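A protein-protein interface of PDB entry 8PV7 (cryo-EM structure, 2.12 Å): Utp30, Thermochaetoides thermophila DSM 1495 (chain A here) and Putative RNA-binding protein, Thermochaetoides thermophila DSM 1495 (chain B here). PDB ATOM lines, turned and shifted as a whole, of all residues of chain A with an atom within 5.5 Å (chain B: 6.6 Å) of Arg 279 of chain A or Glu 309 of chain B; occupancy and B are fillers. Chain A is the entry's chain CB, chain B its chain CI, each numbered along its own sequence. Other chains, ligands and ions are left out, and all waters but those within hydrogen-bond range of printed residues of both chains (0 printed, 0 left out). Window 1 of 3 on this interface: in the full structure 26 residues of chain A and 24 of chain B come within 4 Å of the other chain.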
ATOM      1  N   LEU A  66      -2.575   5.611 -24.271  1.00  0.00           N
ATOM      2  CA  LEU A  66      -2.260   5.874 -22.877  1.00  0.00           C
ATOM      3  C   LEU A  66      -1.906   4.567 -22.194  1.00  0.00           C
ATOM      4  O   LEU A  66      -2.678   3.602 -22.259  1.00  0.00           O
ATOM      5  CB  LEU A  66      -3.440   6.531 -22.160  1.00  0.00           C
ATOM      6  CG  LEU A  66      -3.421   6.454 -20.631  1.00  0.00           C
ATOM      7  CD1 LEU A  66      -2.308   7.306 -20.046  1.00  0.00           C
ATOM      8  CD2 LEU A  66      -4.762   6.861 -20.064  1.00  0.00           C
ATOM      9  N   THR A  67      -0.749   4.542 -21.537  1.00  0.00           N
ATOM     10  CA  THR A  67      -0.310   3.411 -20.736  1.00  0.00           C
ATOM     11  C   THR A  67      -0.284   3.827 -19.274  1.00  0.00           C
ATOM     12  O   THR A  67       0.350   4.825 -18.919  1.00  0.00           O
ATOM     13  CB  THR A  67       1.076   2.933 -21.169  1.00  0.00           C
ATOM     14  OG1 THR A  67       1.022   2.470 -22.523  1.00  0.00           O
ATOM     15  CG2 THR A  67       1.548   1.807 -20.276  1.00  0.00           C
ATOM     16  N   THR A  68      -0.972   3.064 -18.435  1.00  0.00           N
ATOM     17  CA  THR A  68      -1.075   3.343 -17.012  1.00  0.00           C
ATOM     18  C   THR A  68      -0.288   2.313 -16.215  1.00  0.00           C
ATOM     19  O   THR A  68       0.203   1.315 -16.745  1.00  0.00           O
ATOM     20  CB  THR A  68      -2.537   3.354 -16.555  1.00  0.00           C
ATOM     21  OG1 THR A  68      -3.209   2.196 -17.063  1.00  0.00           O
ATOM     22  CG2 THR A  68      -3.242   4.601 -17.053  1.00  0.00           C
ATOM     23  N   LYS A  69      -0.168   2.576 -14.915  1.00  0.00           N
ATOM     24  CA  LYS A  69       0.542   1.672 -14.021  1.00  0.00           C
ATOM     25  C   LYS A  69      -0.337   0.542 -13.508  1.00  0.00           C
ATOM     26  O   LYS A  69       0.173  -0.552 -13.244  1.00  0.00           O
ATOM     27  CB  LYS A  69       1.118   2.461 -12.848  1.00  0.00           C
ATOM     28  CG  LYS A  69       2.068   3.554 -13.278  1.00  0.00           C
ATOM     29  CD  LYS A  69       2.314   4.541 -12.166  1.00  0.00           C
ATOM     30  CE  LYS A  69       3.314   5.593 -12.590  1.00  0.00           C
ATOM     31  NZ  LYS A  69       3.437   6.661 -11.566  1.00  0.00           N
ATOM     32  N   ASN A 277      -0.992   7.958 -11.880  1.00  0.00           N
ATOM     33  CA  ASN A 277      -1.130   6.639 -12.489  1.00  0.00           C
ATOM     34  C   ASN A 277      -0.612   6.623 -13.921  1.00  0.00           C
ATOM     35  O   ASN A 277      -0.370   5.550 -14.484  1.00  0.00           O
ATOM     36  CB  ASN A 277      -2.593   6.209 -12.454  1.00  0.00           C
ATOM     37  CG  ASN A 277      -2.776   4.729 -12.695  1.00  0.00           C
ATOM     38  OD1 ASN A 277      -1.842   3.943 -12.555  1.00  0.00           O
ATOM     39  ND2 ASN A 277      -3.983   4.344 -13.080  1.00  0.00           N
ATOM     40  N   VAL A 278      -0.443   7.795 -14.531  1.00  0.00           N
ATOM     41  CA  VAL A 278      -0.069   7.881 -15.939  1.00  0.00           C
ATOM     42  C   VAL A 278       1.385   7.478 -16.120  1.00  0.00           C
ATOM     43  O   VAL A 278       2.288   8.096 -15.547  1.00  0.00           O
ATOM     44  CB  VAL A 278      -0.310   9.293 -16.498  1.00  0.00           C
ATOM     45  CG1 VAL A 278       0.065   9.342 -17.962  1.00  0.00           C
ATOM     46  CG2 VAL A 278      -1.753   9.694 -16.305  1.00  0.00           C
ATOM     47  N   ARG A 279       1.622   6.428 -16.906  1.00  0.00           N
ATOM     48  CA  ARG A 279       2.993   6.026 -17.192  1.00  0.00           C
ATOM     49  C   ARG A 279       3.472   6.592 -18.524  1.00  0.00           C
ATOM     50  O   ARG A 279       4.415   7.387 -18.564  1.00  0.00           O
ATOM     51  CB  ARG A 279       3.104   4.504 -17.179  1.00  0.00           C
ATOM     52  CG  ARG A 279       4.440   3.960 -17.634  1.00  0.00           C
ATOM     53  CD  ARG A 279       4.314   2.492 -17.972  1.00  0.00           C
ATOM     54  NE  ARG A 279       5.058   1.632 -17.062  1.00  0.00           N
ATOM     55  CZ  ARG A 279       6.191   1.019 -17.371  1.00  0.00           C
ATOM     56  NH1 ARG A 279       6.746   1.153 -18.564  1.00  0.00           N
ATOM     57  NH2 ARG A 279       6.779   0.247 -16.463  1.00  0.00           N
ATOM     58  N   ASN A 280       2.817   6.223 -19.623  1.00  0.00           N
ATOM     59  CA  ASN A 280       3.336   6.526 -20.949  1.00  0.00           C
ATOM     60  C   ASN A 280       2.234   7.107 -21.823  1.00  0.00           C
ATOM     61  O   ASN A 280       1.048   6.828 -21.637  1.00  0.00           O
ATOM     62  CB  ASN A 280       3.920   5.278 -21.617  1.00  0.00           C
ATOM     63  CG  ASN A 280       5.231   4.837 -21.005  1.00  0.00           C
ATOM     64  OD1 ASN A 280       5.842   5.555 -20.220  1.00  0.00           O
ATOM     65  ND2 ASN A 280       5.657   3.630 -21.348  1.00  0.00           N
ATOM     66  N   PHE A 281       2.651   7.903 -22.805  1.00  0.00           N
ATOM     67  CA  PHE A 281       1.743   8.452 -23.804  1.00  0.00           C
ATOM     68  C   PHE A 281       2.408   8.324 -25.165  1.00  0.00           C
ATOM     69  O   PHE A 281       3.549   8.760 -25.337  1.00  0.00           O
ATOM     70  CB  PHE A 281       1.414   9.910 -23.499  1.00  0.00           C
ATOM     71  CG  PHE A 281       0.043  10.115 -22.932  1.00  0.00           C
ATOM     72  CD1 PHE A 281      -1.077   9.700 -23.626  1.00  0.00           C
ATOM     73  CD2 PHE A 281      -0.123  10.733 -21.705  1.00  0.00           C
ATOM     74  CE1 PHE A 281      -2.339   9.889 -23.102  1.00  0.00           C
ATOM     75  CE2 PHE A 281      -1.380  10.928 -21.178  1.00  0.00           C
ATOM     76  CZ  PHE A 281      -2.491  10.506 -21.879  1.00  0.00           C
ATOM     77  N   TYR A 294       4.824  11.672 -23.943  1.00  0.00           N
ATOM     78  CA  TYR A 294       5.051  11.803 -22.513  1.00  0.00           C
ATOM     79  C   TYR A 294       5.537  10.474 -21.969  1.00  0.00           C
ATOM     80  O   TYR A 294       4.971   9.425 -22.287  1.00  0.00           O
ATOM     81  CB  TYR A 294       3.788  12.232 -21.769  1.00  0.00           C
ATOM     82  CG  TYR A 294       3.938  12.166 -20.267  1.00  0.00           C
ATOM     83  CD1 TYR A 294       3.088  11.385 -19.500  1.00  0.00           C
ATOM     84  CD2 TYR A 294       4.935  12.879 -19.618  1.00  0.00           C
ATOM     85  CE1 TYR A 294       3.225  11.317 -18.133  1.00  0.00           C
ATOM     86  CE2 TYR A 294       5.081  12.814 -18.250  1.00  0.00           C
ATOM     87  CZ  TYR A 294       4.222  12.033 -17.513  1.00  0.00           C
ATOM     88  OH  TYR A 294       4.361  11.969 -16.147  1.00  0.00           O
ATOM     89  N   GLN A 295       6.583  10.521 -21.154  1.00  0.00           N
ATOM     90  CA  GLN A 295       7.052   9.347 -20.442  1.00  0.00           C
ATOM     91  C   GLN A 295       7.415   9.759 -19.025  1.00  0.00           C
ATOM     92  O   GLN A 295       7.857  10.883 -18.779  1.00  0.00           O
ATOM     93  CB  GLN A 295       8.240   8.700 -21.155  1.00  0.00           C
ATOM     94  CG  GLN A 295       7.861   7.838 -22.341  1.00  0.00           C
ATOM     95  CD  GLN A 295       9.014   6.999 -22.831  1.00  0.00           C
ATOM     96  OE1 GLN A 295      10.156   7.197 -22.422  1.00  0.00           O
ATOM     97  NE2 GLN A 295       8.724   6.051 -23.712  1.00  0.00           N
ATOM     98  N   THR A 296       7.221   8.839 -18.089  1.00  0.00           N
ATOM     99  CA  THR A 296       7.307   9.154 -16.673  1.00  0.00           C
ATOM    100  C   THR A 296       8.704   8.851 -16.145  1.00  0.00           C
ATOM    101  O   THR A 296       9.511   8.179 -16.796  1.00  0.00           O
ATOM    102  CB  THR A 296       6.249   8.378 -15.891  1.00  0.00           C
ATOM    103  OG1 THR A 296       6.363   8.691 -14.499  1.00  0.00           O
ATOM    104  CG2 THR A 296       6.457   6.888 -16.065  1.00  0.00           C
ATOM    105  N   LEU A 299       8.103   4.659 -11.887  1.00  0.00           N
ATOM    106  CA  LEU A 299       7.486   3.429 -12.359  1.00  0.00           C
ATOM    107  C   LEU A 299       6.560   2.806 -11.329  1.00  0.00           C
ATOM    108  O   LEU A 299       5.987   1.744 -11.590  1.00  0.00           O
ATOM    109  CB  LEU A 299       8.545   2.410 -12.771  1.00  0.00           C
ATOM    110  CG  LEU A 299       9.443   2.773 -13.949  1.00  0.00           C
ATOM    111  CD1 LEU A 299      10.504   1.704 -14.119  1.00  0.00           C
ATOM    112  CD2 LEU A 299       8.634   2.959 -15.219  1.00  0.00           C
ATOM    113  N   VAL B 304      15.478  -4.132 -11.068  1.00  0.00           N
ATOM    114  CA  VAL B 304      15.536  -4.895 -12.316  1.00  0.00           C
ATOM    115  C   VAL B 304      14.466  -4.393 -13.285  1.00  0.00           C
ATOM    116  O   VAL B 304      14.682  -4.349 -14.506  1.00  0.00           O
ATOM    117  CB  VAL B 304      15.432  -6.414 -12.049  1.00  0.00           C
ATOM    118  CG1 VAL B 304      14.316  -6.751 -11.107  1.00  0.00           C
ATOM    119  CG2 VAL B 304      15.316  -7.220 -13.344  1.00  0.00           C
ATOM    120  N   LYS B 305      13.320  -3.941 -12.752  1.00  0.00           N
ATOM    121  CA  LYS B 305      12.325  -3.297 -13.608  1.00  0.00           C
ATOM    122  C   LYS B 305      12.863  -2.014 -14.230  1.00  0.00           C
ATOM    123  O   LYS B 305      12.616  -1.739 -15.409  1.00  0.00           O
ATOM    124  CB  LYS B 305      11.049  -3.001 -12.825  1.00  0.00           C
ATOM    125  CG  LYS B 305      10.151  -4.199 -12.630  1.00  0.00           C
ATOM    126  CD  LYS B 305       9.226  -3.984 -11.457  1.00  0.00           C
ATOM    127  CE  LYS B 305       7.846  -3.559 -11.924  1.00  0.00           C
ATOM    128  NZ  LYS B 305       7.295  -4.502 -12.934  1.00  0.00           N
ATOM    129  N   VAL B 306      13.611  -1.223 -13.456  1.00  0.00           N
ATOM    130  CA  VAL B 306      14.204   0.004 -13.979  1.00  0.00           C
ATOM    131  C   VAL B 306      15.231  -0.318 -15.061  1.00  0.00           C
ATOM    132  O   VAL B 306      15.283   0.341 -16.103  1.00  0.00           O
ATOM    133  CB  VAL B 306      14.809   0.832 -12.827  1.00  0.00           C
ATOM    134  CG1 VAL B 306      15.978   1.692 -13.295  1.00  0.00           C
ATOM    135  CG2 VAL B 306      13.741   1.706 -12.194  1.00  0.00           C
ATOM    136  N   ALA B 307      16.050  -1.351 -14.840  1.00  0.00           N
ATOM    137  CA  ALA B 307      17.041  -1.738 -15.845  1.00  0.00           C
ATOM    138  C   ALA B 307      16.369  -2.172 -17.145  1.00  0.00           C
ATOM    139  O   ALA B 307      16.766  -1.743 -18.240  1.00  0.00           O
ATOM    140  CB  ALA B 307      17.930  -2.853 -15.300  1.00  0.00           C
ATOM    141  N   LYS B 308      15.313  -2.983 -17.033  1.00  0.00           N
ATOM    142  CA  LYS B 308      14.545  -3.393 -18.206  1.00  0.00           C
ATOM    143  C   LYS B 308      13.897  -2.197 -18.891  1.00  0.00           C
ATOM    144  O   LYS B 308      13.761  -2.162 -20.118  1.00  0.00           O
ATOM    145  CB  LYS B 308      13.481  -4.412 -17.794  1.00  0.00           C
ATOM    146  CG  LYS B 308      12.892  -5.220 -18.940  1.00  0.00           C
ATOM    147  CD  LYS B 308      11.948  -6.293 -18.413  1.00  0.00           C
ATOM    148  CE  LYS B 308      11.040  -6.833 -19.508  1.00  0.00           C
ATOM    149  NZ  LYS B 308       9.606  -6.549 -19.218  1.00  0.00           N
ATOM    150  N   GLU B 309      13.503  -1.197 -18.103  1.00  0.00           N
ATOM    151  CA  GLU B 309      12.762  -0.071 -18.648  1.00  0.00           C
ATOM    152  C   GLU B 309      13.713   0.839 -19.432  1.00  0.00           C
ATOM    153  O   GLU B 309      13.378   1.309 -20.525  1.00  0.00           O
ATOM    154  CB  GLU B 309      12.089   0.657 -17.479  1.00  0.00           C
ATOM    155  CG  GLU B 309      11.176   1.836 -17.757  1.00  0.00           C
ATOM    156  CD  GLU B 309      10.582   1.826 -19.148  1.00  0.00           C
ATOM    157  OE1 GLU B 309       9.606   1.077 -19.367  1.00  0.00           O
ATOM    158  OE2 GLU B 309      11.013   2.621 -19.994  1.00  0.00           O
ATOM    159  N   GLU B 310      14.927   1.053 -18.898  1.00  0.00           N
ATOM    160  CA  GLU B 310      16.007   1.688 -19.661  1.00  0.00           C
ATOM    161  C   GLU B 310      16.322   0.949 -20.954  1.00  0.00           C
ATOM    162  O   GLU B 310      16.510   1.586 -22.000  1.00  0.00           O
ATOM    163  CB  GLU B 310      17.288   1.797 -18.827  1.00  0.00           C
ATOM    164  CG  GLU B 310      17.594   3.082 -18.018  1.00  0.00           C
ATOM    165  CD  GLU B 310      16.507   3.641 -17.125  1.00  0.00           C
ATOM    166  OE1 GLU B 310      16.619   4.839 -16.788  1.00  0.00           O
ATOM    167  OE2 GLU B 310      15.562   2.935 -16.746  1.00  0.00           O
ATOM    168  N   GLN B 311      16.427  -0.385 -20.903  1.00  0.00           N
ATOM    169  CA  GLN B 311      16.713  -1.126 -22.132  1.00  0.00           C
ATOM    170  C   GLN B 311      15.594  -0.972 -23.156  1.00  0.00           C
ATOM    171  O   GLN B 311      15.859  -0.800 -24.353  1.00  0.00           O
ATOM    172  CB  GLN B 311      16.973  -2.606 -21.840  1.00  0.00           C
ATOM    173  CG  GLN B 311      18.212  -2.882 -21.000  1.00  0.00           C
ATOM    174  CD  GLN B 311      18.091  -4.133 -20.151  1.00  0.00           C
ATOM    175  OE1 GLN B 311      18.201  -4.083 -18.928  1.00  0.00           O
ATOM    176  NE2 GLN B 311      17.855  -5.266 -20.801  1.00  0.00           N
ATOM    177  N   ARG B 312      14.341  -1.003 -22.702  1.00  0.00           N
ATOM    178  CA  ARG B 312      13.218  -0.858 -23.620  1.00  0.00           C
ATOM    179  C   ARG B 312      13.175   0.542 -24.227  1.00  0.00           C
ATOM    180  O   ARG B 312      12.886   0.701 -25.419  1.00  0.00           O
ATOM    181  CB  ARG B 312      11.915  -1.185 -22.891  1.00  0.00           C
ATOM    182  CG  ARG B 312      10.823  -1.751 -23.776  1.00  0.00           C
ATOM    183  CD  ARG B 312       9.450  -1.419 -23.224  1.00  0.00           C
ATOM    184  NE  ARG B 312       8.880  -2.520 -22.459  1.00  0.00           N
ATOM    185  CZ  ARG B 312       8.426  -2.410 -21.218  1.00  0.00           C
ATOM    186  NH1 ARG B 312       8.477  -1.264 -20.562  1.00  0.00           N
ATOM    187  NH2 ARG B 312       7.904  -3.478 -20.621  1.00  0.00           N
ATOM    188  N   ARG B 313      13.480   1.567 -23.423  1.00  0.00           N
ATOM    189  CA  ARG B 313      13.554   2.933 -23.937  1.00  0.00           C
ATOM    190  C   ARG B 313      14.672   3.096 -24.954  1.00  0.00           C
ATOM    191  O   ARG B 313      14.489   3.774 -25.968  1.00  0.00           O
ATOM    192  CB  ARG B 313      13.748   3.918 -22.791  1.00  0.00           C
ATOM    193  CG  ARG B 313      12.468   4.453 -22.200  1.00  0.00           C
ATOM    194  CD  ARG B 313      12.757   5.188 -20.905  1.00  0.00           C
ATOM    195  NE  ARG B 313      11.775   6.207 -20.552  1.00  0.00           N
ATOM    196  CZ  ARG B 313      10.925   6.110 -19.540  1.00  0.00           C
ATOM    197  NH1 ARG B 313      10.724   4.966 -18.912  1.00  0.00           N
ATOM    198  NH2 ARG B 313      10.249   7.185 -19.154  1.00  0.00           N
ATOM    199  N   ALA B 314      15.840   2.504 -24.695  1.00  0.00           N
ATOM    200  CA  ALA B 314      16.937   2.597 -25.652  1.00  0.00           C
ATOM    201  C   ALA B 314      16.573   1.911 -26.963  1.00  0.00           C
ATOM    202  O   ALA B 314      16.836   2.446 -28.054  1.00  0.00           O
ATOM    203  CB  ALA B 314      18.205   1.987 -25.058  1.00  0.00           C
ATOM    204  N   ARG B 316      13.517   1.391 -28.183  1.00  0.00           N
ATOM    205  CA  ARG B 316      12.543   2.233 -28.862  1.00  0.00           C
ATOM    206  C   ARG B 316      13.215   3.454 -29.471  1.00  0.00           C
ATOM    207  O   ARG B 316      12.831   3.908 -30.549  1.00  0.00           O
ATOM    208  CB  ARG B 316      11.439   2.656 -27.890  1.00  0.00           C
ATOM    209  CG  ARG B 316      10.211   3.245 -28.576  1.00  0.00           C
ATOM    210  CD  ARG B 316       9.117   3.641 -27.592  1.00  0.00           C
ATOM    211  NE  ARG B 316       9.314   3.064 -26.268  1.00  0.00           N
ATOM    212  CZ  ARG B 316       8.701   1.980 -25.814  1.00  0.00           C
ATOM    213  NH1 ARG B 316       7.866   1.289 -26.570  1.00  0.00           N
ATOM    214  NH2 ARG B 316       8.933   1.581 -24.569  1.00  0.00           N
ATOM    215  N   LEU B 332      14.777   7.650 -15.240  1.00  0.00           N
ATOM    216  CA  LEU B 332      14.042   6.945 -14.199  1.00  0.00           C
ATOM    217  C   LEU B 332      14.786   7.035 -12.876  1.00  0.00           C
ATOM    218  O   LEU B 332      15.869   6.461 -12.722  1.00  0.00           O
ATOM    219  CB  LEU B 332      13.837   5.483 -14.603  1.00  0.00           C
ATOM    220  CG  LEU B 332      12.826   5.113 -15.695  1.00  0.00           C
ATOM    221  CD1 LEU B 332      11.596   5.968 -15.593  1.00  0.00           C
ATOM    222  CD2 LEU B 332      13.413   5.270 -17.078  1.00  0.00           C
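The backbone carbonyl oxygen of Thr 67 of chain A is in hydrogen-bond range of the backbone NH of Arg 279 of chain A (2.9 Å).
The backbone carbonyl oxygen (O) of Arg 279 of chain A lies within hydrogen-bond range of the backbone NH (N) of Thr 296 of chain A (3.2 Å).
The side-chain carboxylate (OE2) of Glu 310 of chain B sits close to the backbone carbonyl oxygen (O) of Val 306 of chain B, at 2.7 Å.
OE1 of Glu 309 of chain B is in salt-bridge range of NH1 of Arg 312 of chain B (2.9 Å).
The side-chain carboxylate (OE2) of Glu 309 of chain B is in salt-bridge range of the guanidinium group (NH1) of Arg 313 of chain B, at 2.6 Å.
NH1 of Arg 312 of chain B touches NH1 of Arg 279 of chain A (3.6 Å).
NE2 of Gln 295 of chain A touches NE of Arg 316 of chain B (3.98 Å).
Thr 296 of chain A touches Leu 332 of chain B.
Val 306 of chain B touches Leu 299 of chain A.
Glu 309 of chain B touches Leu 299 of chain A (CG to CD1, 3.7 Å).
The guanidinium group (NH1) of Arg 279 of chain A lies within salt-bridge range of the side-chain carboxylate (OE1) of Glu 309 of chain B.
The side-chain amide oxygen (OE1) of Gln 295 of chain A sits at hydrogen-bond distance from the guanidinium group (NE) of Arg 313 of chain B, at 2.7 Å.
The guanidinium group (NH2) of Arg 313 of chain B sits at hydrogen-bond distance from the backbone carbonyl oxygen (O) of Thr 296 of chain A.
Arg 279 of chain A touches just these residues of chain B: Glu 309 (3.0 Å) and Arg 312 (3.6 Å).
Glu 309 of chain B touches two residues of chain A.
Printed residues of chain B within 4 Å of Thr 296 of chain A: Arg 313 and Leu 332.
Of the printed residues of chain A, Arg 316 of chain B touches Gln 295.
Of the printed residues of chain A, Val 306 of chain B touches Leu 299.
Gln 311 of chain B touches none of the printed residues of chain A.
Ala 314 of chain B touches none of the printed residues of chain A.
The nearest residue of chain B that does not touch Arg 279 of chain A is Arg 313 of chain B (5.5 Å).
Of the 13 printed residues of chain A, 4 touch a printed residue of chain B.
Of the 13 printed residues of chain B, 6 touch a printed residue of chain A.
Hydrophobic or aromatic side chains of chain B that line the printed part of chain A: Val 306 and Leu 332.
Among the printed residues, Asp or Glu carboxylates within 4 Å of a Lys or Arg side-chain nitrogen of the other chain: Arg 279 of chain A with Glu 309 of chain B (3.0 Å).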
